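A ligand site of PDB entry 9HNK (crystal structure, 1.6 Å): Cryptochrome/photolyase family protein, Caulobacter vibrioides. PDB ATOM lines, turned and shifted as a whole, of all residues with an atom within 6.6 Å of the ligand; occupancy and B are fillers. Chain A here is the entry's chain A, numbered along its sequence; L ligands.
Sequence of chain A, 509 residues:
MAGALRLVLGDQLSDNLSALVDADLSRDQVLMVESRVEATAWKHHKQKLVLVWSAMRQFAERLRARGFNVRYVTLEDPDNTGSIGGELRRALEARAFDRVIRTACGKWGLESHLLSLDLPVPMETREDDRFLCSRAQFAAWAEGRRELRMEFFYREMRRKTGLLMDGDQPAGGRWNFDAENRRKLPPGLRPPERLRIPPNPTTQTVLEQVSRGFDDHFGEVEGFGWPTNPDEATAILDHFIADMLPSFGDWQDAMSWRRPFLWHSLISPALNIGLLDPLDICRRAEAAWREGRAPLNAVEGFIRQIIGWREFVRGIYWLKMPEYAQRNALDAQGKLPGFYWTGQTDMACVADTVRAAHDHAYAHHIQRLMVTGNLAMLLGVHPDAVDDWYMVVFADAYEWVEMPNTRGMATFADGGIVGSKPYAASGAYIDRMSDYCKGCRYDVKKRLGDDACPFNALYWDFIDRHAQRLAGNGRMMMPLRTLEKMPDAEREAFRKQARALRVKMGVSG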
ATOM      1  N   ASP A 346     -10.520   2.380  11.081  1.00  0.00           N
ATOM      2  CA  ASP A 346     -11.002   1.922   9.778  1.00  0.00           C
ATOM      3  C   ASP A 346     -11.304   0.432   9.794  1.00  0.00           C
ATOM      4  O   ASP A 346     -11.918  -0.061   8.846  1.00  0.00           O
ATOM      5  CB  ASP A 346      -9.950   2.169   8.707  1.00  0.00           C
ATOM      6  CG  ASP A 346      -9.916   3.624   8.254  1.00  0.00           C
ATOM      7  OD1 ASP A 346      -9.059   4.010   7.426  1.00  0.00           O
ATOM      8  OD2 ASP A 346     -10.737   4.402   8.794  1.00  0.00           O
ATOM      9  N   MET A 347     -10.896  -0.310  10.830  1.00  0.00           N
ATOM     10  CA  MET A 347     -11.306  -1.726  10.895  1.00  0.00           C
ATOM     11  C   MET A 347     -12.785  -1.815  11.225  1.00  0.00           C
ATOM     12  O   MET A 347     -13.183  -1.618  12.376  1.00  0.00           O
ATOM     13  CB  MET A 347     -10.472  -2.485  11.931  1.00  0.00           C
ATOM     14  CG  MET A 347      -8.985  -2.483  11.599  1.00  0.00           C
ATOM     15  SD  MET A 347      -8.062  -3.477  12.828  1.00  0.00           S
ATOM     16  CE  MET A 347      -7.887  -2.244  14.070  1.00  0.00           C
ATOM     17  N   ALA A 348     -13.603  -2.207  10.231  1.00  0.00           N
ATOM     18  CA  ALA A 348     -15.052  -2.130  10.399  1.00  0.00           C
ATOM     19  C   ALA A 348     -15.547  -3.063  11.482  1.00  0.00           C
ATOM     20  O   ALA A 348     -16.470  -2.704  12.229  1.00  0.00           O
ATOM     21  CB  ALA A 348     -15.747  -2.436   9.097  1.00  0.00           C
ATOM     22  N   CYS A 349     -14.961  -4.256  11.566  1.00  0.00           N
ATOM     23  CA  CYS A 349     -15.398  -5.215  12.556  1.00  0.00           C
ATOM     24  C   CYS A 349     -15.125  -4.675  13.964  1.00  0.00           C
ATOM     25  O   CYS A 349     -15.976  -4.794  14.848  1.00  0.00           O
ATOM     26  CB  CYS A 349     -14.658  -6.529  12.312  1.00  0.00           C
ATOM     27  SG  CYS A 349     -12.822  -6.349  12.225  1.00  0.00           S
ATOM     28  N   VAL A 350     -13.939  -4.074  14.186  1.00  0.00           N
ATOM     29  CA  VAL A 350     -13.604  -3.566  15.508  1.00  0.00           C
ATOM     30  C   VAL A 350     -14.473  -2.395  15.830  1.00  0.00           C
ATOM     31  O   VAL A 350     -14.959  -2.267  16.956  1.00  0.00           O
ATOM     32  CB  VAL A 350     -12.113  -3.235  15.577  1.00  0.00           C
ATOM     33  CG1 VAL A 350     -11.731  -2.562  16.877  1.00  0.00           C
ATOM     34  CG2 VAL A 350     -11.232  -4.478  15.352  1.00  0.00           C
ATOM     35  N   VAL A 371     -12.950 -10.837  17.583  1.00  0.00           N
ATOM     36  CA  VAL A 371     -12.672  -9.501  17.039  1.00  0.00           C
ATOM     37  C   VAL A 371     -11.761  -8.747  18.009  1.00  0.00           C
ATOM     38  O   VAL A 371     -10.543  -8.686  17.788  1.00  0.00           O
ATOM     39  CB  VAL A 371     -13.957  -8.718  16.713  1.00  0.00           C
ATOM     40  CG1 VAL A 371     -13.624  -7.359  16.119  1.00  0.00           C
ATOM     41  CG2 VAL A 371     -14.801  -9.496  15.714  1.00  0.00           C
ATOM     42  N   SER A 426      -6.947 -14.885  11.392  1.00  0.00           N
ATOM     43  CA  SER A 426      -6.731 -13.803  10.445  1.00  0.00           C
ATOM     44  C   SER A 426      -8.087 -13.204  10.054  1.00  0.00           C
ATOM     45  O   SER A 426      -9.159 -13.595  10.571  1.00  0.00           O
ATOM     46  CB  SER A 426      -5.975 -14.292   9.210  1.00  0.00           C
ATOM     47  OG  SER A 426      -6.871 -15.160   8.473  1.00  0.00           O
ATOM     48  N   GLY A 427      -8.047 -12.238   9.150  1.00  0.00           N
ATOM     49  CA  GLY A 427      -9.246 -11.605   8.689  1.00  0.00           C
ATOM     50  C   GLY A 427     -10.138 -12.563   7.935  1.00  0.00           C
ATOM     51  O   GLY A 427     -11.364 -12.342   7.849  1.00  0.00           O
ATOM     52  N   ALA A 428      -9.562 -13.645   7.402  1.00  0.00           N
ATOM     53  CA  ALA A 428     -10.372 -14.657   6.709  1.00  0.00           C
ATOM     54  C   ALA A 428     -11.479 -15.194   7.600  1.00  0.00           C
ATOM     55  O   ALA A 428     -12.586 -15.510   7.124  1.00  0.00           O
ATOM     56  CB  ALA A 428      -9.483 -15.807   6.207  1.00  0.00           C
ATOM     57  N   ILE A 430     -13.049 -13.600  10.127  1.00  0.00           N
ATOM     58  CA  ILE A 430     -14.085 -12.586  10.287  1.00  0.00           C
ATOM     59  C   ILE A 430     -14.875 -12.453   8.991  1.00  0.00           C
ATOM     60  O   ILE A 430     -16.109 -12.321   9.015  1.00  0.00           O
ATOM     61  CB  ILE A 430     -13.472 -11.251  10.751  1.00  0.00           C
ATOM     62  CG1 ILE A 430     -12.898 -11.445  12.150  1.00  0.00           C
ATOM     63  CG2 ILE A 430     -14.533 -10.117  10.708  1.00  0.00           C
ATOM     64  CD1 ILE A 430     -12.049 -10.255  12.672  1.00  0.00           C
ATOM     65  N   ASP A 431     -14.196 -12.590   7.854  1.00  0.00           N
ATOM     66  CA  ASP A 431     -14.865 -12.496   6.554  1.00  0.00           C
ATOM     67  C   ASP A 431     -15.859 -13.617   6.395  1.00  0.00           C
ATOM     68  O   ASP A 431     -16.979 -13.394   5.921  1.00  0.00           O
ATOM     69  CB  ASP A 431     -13.842 -12.522   5.421  1.00  0.00           C
ATOM     70  CG  ASP A 431     -14.459 -12.261   4.063  1.00  0.00           C
ATOM     71  OD1 ASP A 431     -15.442 -11.480   3.952  1.00  0.00           O
ATOM     72  OD2 ASP A 431     -13.973 -12.858   3.058  1.00  0.00           O
ATOM     73  N   SER A 434     -19.038 -12.987   8.969  1.00  0.00           N
ATOM     74  CA  SER A 434     -19.671 -11.683   9.065  1.00  0.00           C
ATOM     75  C   SER A 434     -19.943 -11.098   7.693  1.00  0.00           C
ATOM     76  O   SER A 434     -19.526 -11.630   6.663  1.00  0.00           O
ATOM     77  CB  SER A 434     -18.809 -10.691   9.797  1.00  0.00           C
ATOM     78  OG  SER A 434     -17.793 -10.249   8.939  1.00  0.00           O
ATOM     79  N   TYR A 436     -18.832  -7.892   7.291  1.00  0.00           N
ATOM     80  CA  TYR A 436     -18.102  -6.664   7.542  1.00  0.00           C
ATOM     81  C   TYR A 436     -17.169  -6.304   6.403  1.00  0.00           C
ATOM     82  O   TYR A 436     -16.965  -5.111   6.099  1.00  0.00           O
ATOM     83  CB  TYR A 436     -17.228  -6.799   8.820  1.00  0.00           C
ATOM     84  CG  TYR A 436     -17.927  -6.728  10.120  1.00  0.00           C
ATOM     85  CD1 TYR A 436     -18.760  -5.662  10.431  1.00  0.00           C
ATOM     86  CD2 TYR A 436     -17.732  -7.694  11.092  1.00  0.00           C
ATOM     87  CE1 TYR A 436     -19.388  -5.597  11.633  1.00  0.00           C
ATOM     88  CE2 TYR A 436     -18.328  -7.619  12.280  1.00  0.00           C
ATOM     89  CZ  TYR A 436     -19.200  -6.613  12.554  1.00  0.00           C
ATOM     90  OH  TYR A 436     -19.821  -6.543  13.790  1.00  0.00           O
ATOM     91  N   CYS A 437     -16.514  -7.303   5.799  1.00  0.00           N
ATOM     92  CA  CYS A 437     -15.287  -6.988   5.057  1.00  0.00           C
ATOM     93  C   CYS A 437     -15.573  -6.253   3.761  1.00  0.00           C
ATOM     94  O   CYS A 437     -14.726  -5.465   3.291  1.00  0.00           O
ATOM     95  CB  CYS A 437     -14.499  -8.261   4.821  1.00  0.00           C
ATOM     96  SG  CYS A 437     -14.010  -9.012   6.378  1.00  0.00           S
ATOM     97  N   LYS A 438     -16.705  -6.517   3.110  1.00  0.00           N
ATOM     98  CA  LYS A 438     -17.007  -5.814   1.876  1.00  0.00           C
ATOM     99  C   LYS A 438     -17.112  -4.320   2.104  1.00  0.00           C
ATOM    100  O   LYS A 438     -16.573  -3.521   1.329  1.00  0.00           O
ATOM    101  CB  LYS A 438     -18.308  -6.357   1.284  1.00  0.00           C
ATOM    102  CG  LYS A 438     -18.743  -5.729  -0.029  1.00  0.00           C
ATOM    103  CD  LYS A 438     -17.568  -5.272  -0.895  1.00  0.00           C
ATOM    104  CE  LYS A 438     -18.010  -5.054  -2.356  1.00  0.00           C
ATOM    105  NZ  LYS A 438     -19.491  -4.983  -2.508  1.00  0.00           N
ATOM    106  N   CYS A 440     -15.791  -2.681   4.589  1.00  0.00           N
ATOM    107  CA  CYS A 440     -14.572  -2.185   5.212  1.00  0.00           C
ATOM    108  C   CYS A 440     -13.617  -1.649   4.151  1.00  0.00           C
ATOM    109  O   CYS A 440     -13.495  -2.190   3.056  1.00  0.00           O
ATOM    110  CB  CYS A 440     -13.897  -3.333   5.938  1.00  0.00           C
ATOM    111  SG  CYS A 440     -12.454  -2.901   6.940  1.00  0.00           S
ATOM    112  N   ARG A 441     -12.925  -0.545   4.463  1.00  0.00           N
ATOM    113  CA  ARG A 441     -11.990  -0.011   3.467  1.00  0.00           C
ATOM    114  C   ARG A 441     -10.800  -0.947   3.239  1.00  0.00           C
ATOM    115  O   ARG A 441     -10.194  -0.905   2.157  1.00  0.00           O
ATOM    116  CB  ARG A 441     -11.521   1.394   3.904  1.00  0.00           C
ATOM    117  CG  ARG A 441     -10.442   1.337   4.953  1.00  0.00           C
ATOM    118  CD  ARG A 441      -9.066   1.481   4.375  1.00  0.00           C
ATOM    119  NE  ARG A 441      -8.165   2.196   5.276  1.00  0.00           N
ATOM    120  CZ  ARG A 441      -6.846   2.130   5.205  1.00  0.00           C
ATOM    121  NH1 ARG A 441      -6.235   1.633   4.128  1.00  0.00           N
ATOM    122  NH2 ARG A 441      -6.117   2.575   6.230  1.00  0.00           N
ATOM    123  N   TYR A 442     -10.481  -1.801   4.203  1.00  0.00           N
ATOM    124  CA  TYR A 442      -9.373  -2.715   4.032  1.00  0.00           C
ATOM    125  C   TYR A 442      -9.753  -3.872   3.122  1.00  0.00           C
ATOM    126  O   TYR A 442     -10.926  -4.221   2.951  1.00  0.00           O
ATOM    127  CB  TYR A 442      -8.897  -3.277   5.368  1.00  0.00           C
ATOM    128  CG  TYR A 442      -8.196  -2.285   6.297  1.00  0.00           C
ATOM    129  CD1 TYR A 442      -6.967  -1.754   5.964  1.00  0.00           C
ATOM    130  CD2 TYR A 442      -8.781  -1.912   7.469  1.00  0.00           C
ATOM    131  CE1 TYR A 442      -6.317  -0.882   6.831  1.00  0.00           C
ATOM    132  CE2 TYR A 442      -8.159  -1.008   8.344  1.00  0.00           C
ATOM    133  CZ  TYR A 442      -6.947  -0.499   8.001  1.00  0.00           C
ATOM    134  OH  TYR A 442      -6.331   0.344   8.897  1.00  0.00           O
ATOM    135  N   ASP A 443      -8.721  -4.468   2.516  1.00  0.00           N
ATOM    136  CA  ASP A 443      -8.854  -5.640   1.632  1.00  0.00           C
ATOM    137  C   ASP A 443      -8.476  -6.873   2.447  1.00  0.00           C
ATOM    138  O   ASP A 443      -7.301  -7.072   2.785  1.00  0.00           O
ATOM    139  CB  ASP A 443      -7.967  -5.489   0.414  1.00  0.00           C
ATOM    140  CG  ASP A 443      -8.189  -6.574  -0.642  1.00  0.00           C
ATOM    141  OD1 ASP A 443      -8.811  -7.620  -0.333  1.00  0.00           O
ATOM    142  OD2 ASP A 443      -7.755  -6.368  -1.811  1.00  0.00           O
ATOM    143  N   VAL A 444      -9.476  -7.700   2.741  1.00  0.00           N
ATOM    144  CA  VAL A 444      -9.270  -8.893   3.552  1.00  0.00           C
ATOM    145  C   VAL A 444      -8.491  -9.979   2.821  1.00  0.00           C
ATOM    146  O   VAL A 444      -8.086 -10.950   3.449  1.00  0.00           O
ATOM    147  CB  VAL A 444     -10.640  -9.429   4.060  1.00  0.00           C
ATOM    148  CG1 VAL A 444     -11.405 -10.130   2.949  1.00  0.00           C
ATOM    149  CG2 VAL A 444     -10.466 -10.328   5.260  1.00  0.00           C
ATOM    150  N   LYS A 445      -8.258  -9.822   1.518  1.00  0.00           N
ATOM    151  CA  LYS A 445      -7.437 -10.775   0.782  1.00  0.00           C
ATOM    152  C   LYS A 445      -5.961 -10.400   0.758  1.00  0.00           C
ATOM    153  O   LYS A 445      -5.156 -11.180   0.246  1.00  0.00           O
ATOM    154  CB  LYS A 445      -7.922 -10.921  -0.678  1.00  0.00           C
ATOM    155  CG  LYS A 445      -9.447 -11.194  -0.807  1.00  0.00           C
ATOM    156  CD  LYS A 445      -9.956 -10.616  -2.150  1.00  0.00           C
ATOM    157  CE  LYS A 445     -11.250  -9.820  -1.945  1.00  0.00           C
ATOM    158  NZ  LYS A 445     -10.981  -8.363  -1.734  1.00  0.00           N
ATOM    159  N   ALA A 452      -4.063  -3.504   3.305  1.00  0.00           N
ATOM    160  CA  ALA A 452      -4.260  -4.870   3.835  1.00  0.00           C
ATOM    161  C   ALA A 452      -5.008  -4.892   5.153  1.00  0.00           C
ATOM    162  O   ALA A 452      -4.724  -4.100   6.070  1.00  0.00           O
ATOM    163  CB  ALA A 452      -2.926  -5.550   4.016  1.00  0.00           C
ATOM    164  N   CYS A 453      -5.985  -5.779   5.261  1.00  0.00           N
ATOM    165  CA  CYS A 453      -6.610  -6.088   6.551  1.00  0.00           C
ATOM    166  C   CYS A 453      -5.533  -6.311   7.636  1.00  0.00           C
ATOM    167  O   CYS A 453      -4.699  -7.221   7.500  1.00  0.00           O
ATOM    168  CB  CYS A 453      -7.491  -7.330   6.455  1.00  0.00           C
ATOM    169  SG  CYS A 453      -8.084  -7.900   8.056  1.00  0.00           S
ATOM    170  N   PRO A 454      -5.493  -5.488   8.680  1.00  0.00           N
ATOM    171  CA  PRO A 454      -4.408  -5.653   9.689  1.00  0.00           C
ATOM    172  C   PRO A 454      -4.374  -7.019  10.324  1.00  0.00           C
ATOM    173  O   PRO A 454      -3.313  -7.452  10.762  1.00  0.00           O
ATOM    174  CB  PRO A 454      -4.721  -4.576  10.720  1.00  0.00           C
ATOM    175  CG  PRO A 454      -5.452  -3.556   9.929  1.00  0.00           C
ATOM    176  CD  PRO A 454      -6.296  -4.302   8.949  1.00  0.00           C
ATOM    177  N   PHE A 455      -5.534  -7.682  10.487  1.00  0.00           N
ATOM    178  CA  PHE A 455      -5.538  -8.980  11.126  1.00  0.00           C
ATOM    179  C   PHE A 455      -4.675 -10.008  10.392  1.00  0.00           C
ATOM    180  O   PHE A 455      -4.250 -11.021  10.992  1.00  0.00           O
ATOM    181  CB  PHE A 455      -6.955  -9.547  11.195  1.00  0.00           C
ATOM    182  CG  PHE A 455      -7.828  -8.992  12.291  1.00  0.00           C
ATOM    183  CD1 PHE A 455      -8.580  -7.834  12.046  1.00  0.00           C
ATOM    184  CD2 PHE A 455      -7.942  -9.637  13.512  1.00  0.00           C
ATOM    185  CE1 PHE A 455      -9.413  -7.350  13.030  1.00  0.00           C
ATOM    186  CE2 PHE A 455      -8.816  -9.173  14.490  1.00  0.00           C
ATOM    187  CZ  PHE A 455      -9.540  -8.037  14.248  1.00  0.00           C
ATOM    188  N   ASN A 456      -4.424  -9.807   9.109  1.00  0.00           N
ATOM    189  CA  ASN A 456      -3.713 -10.822   8.340  1.00  0.00           C
ATOM    190  C   ASN A 456      -2.226 -10.819   8.689  1.00  0.00           C
ATOM    191  O   ASN A 456      -1.673 -11.855   9.026  1.00  0.00           O
ATOM    192  CB  ASN A 456      -3.944 -10.584   6.835  1.00  0.00           C
ATOM    193  CG  ASN A 456      -5.370 -10.962   6.407  1.00  0.00           C
ATOM    194  OD1 ASN A 456      -6.057 -11.699   7.098  1.00  0.00           O
ATOM    195  ND2 ASN A 456      -5.778 -10.450   5.284  1.00  0.00           N
HETATM  196 FE1  LIG L   1     -12.721  -7.545   7.540  1.00  0.00          FE
HETATM  197 FE2  LIG L   1     -10.186  -6.966   8.210  1.00  0.00          FE
HETATM  198 FE3  LIG L   1     -12.173  -6.486   9.990  1.00  0.00          FE
HETATM  199 FE4  LIG L   1     -11.923  -4.923   7.786  1.00  0.00          FE
HETATM  200  S1  LIG L   1     -10.447  -5.073   9.435  1.00  0.00           S
HETATM  201  S2  LIG L   1     -13.859  -5.824   8.624  1.00  0.00           S
HETATM  202  S3  LIG L   1     -11.185  -6.474   6.276  1.00  0.00           S
HETATM  203  S4  LIG L   1     -11.549  -8.468   9.194  1.00  0.00           S
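An iron atom (FE4) of the ligand is bound by the side-chain sulfur (SG) of Cys 440 (2.3 Å). FE1 of the ligand is bound by SG of Cys 437, at 2.3 Å. The side-chain sulfur of Cys 453 is bound to an iron atom (FE2) of the ligand (2.3 Å). The backbone NH (N) of Cys 349 sits close to a sulfur (S2) of the ligand (3.5 Å). The side-chain sulfur (SG) of Cys 349 is bound to an iron atom (FE3) of the ligand.
SG of Cys 440 lies close to N of Ala 348 (3.6 Å). The side-chain sulfur of Cys 440 lies close to the backbone NH of Tyr 442, at 3.5 Å. The side-chain sulfur (SG) of Cys 440 sits close to the backbone carbonyl oxygen (O) of Asp 346, 3.5 Å away. The side-chain sulfur (SG) of Cys 437 lies close to the side-chain carboxylate (OD1) of Asp 431 (3.7 Å). The side-chain sulfur (SG) of Cys 453 sits close to the backbone NH (N) of Phe 455. O of Asp 443 lies within hydrogen-bond range of N of Cys 453 (3.1 Å). N of Tyr 436 lies within hydrogen-bond range of OG of Ser 434, 3.1 Å away. The backbone carbonyl oxygen (O) of Ile 430 is in hydrogen-bond range of the side-chain hydroxyl (OG) of Ser 434 (2.7 Å).
Met 347 touches the ligand (CB to S1, 3.6 Å). Ala 348 touches the ligand (CB to S2, 3.9 Å). Gly 427 touches the ligand (CA to S4, 3.9 Å). Ile 430 touches the ligand. CB of Tyr 436 touches S2 of the ligand, 3.5 Å away. CB of Val 444 touches S3 of the ligand (3.7 Å). Of the 26 residues printed, 10 come within 4 Å of the ligand. The nearest printed residue that does not touch the ligand is Tyr 442 (4.02 Å).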
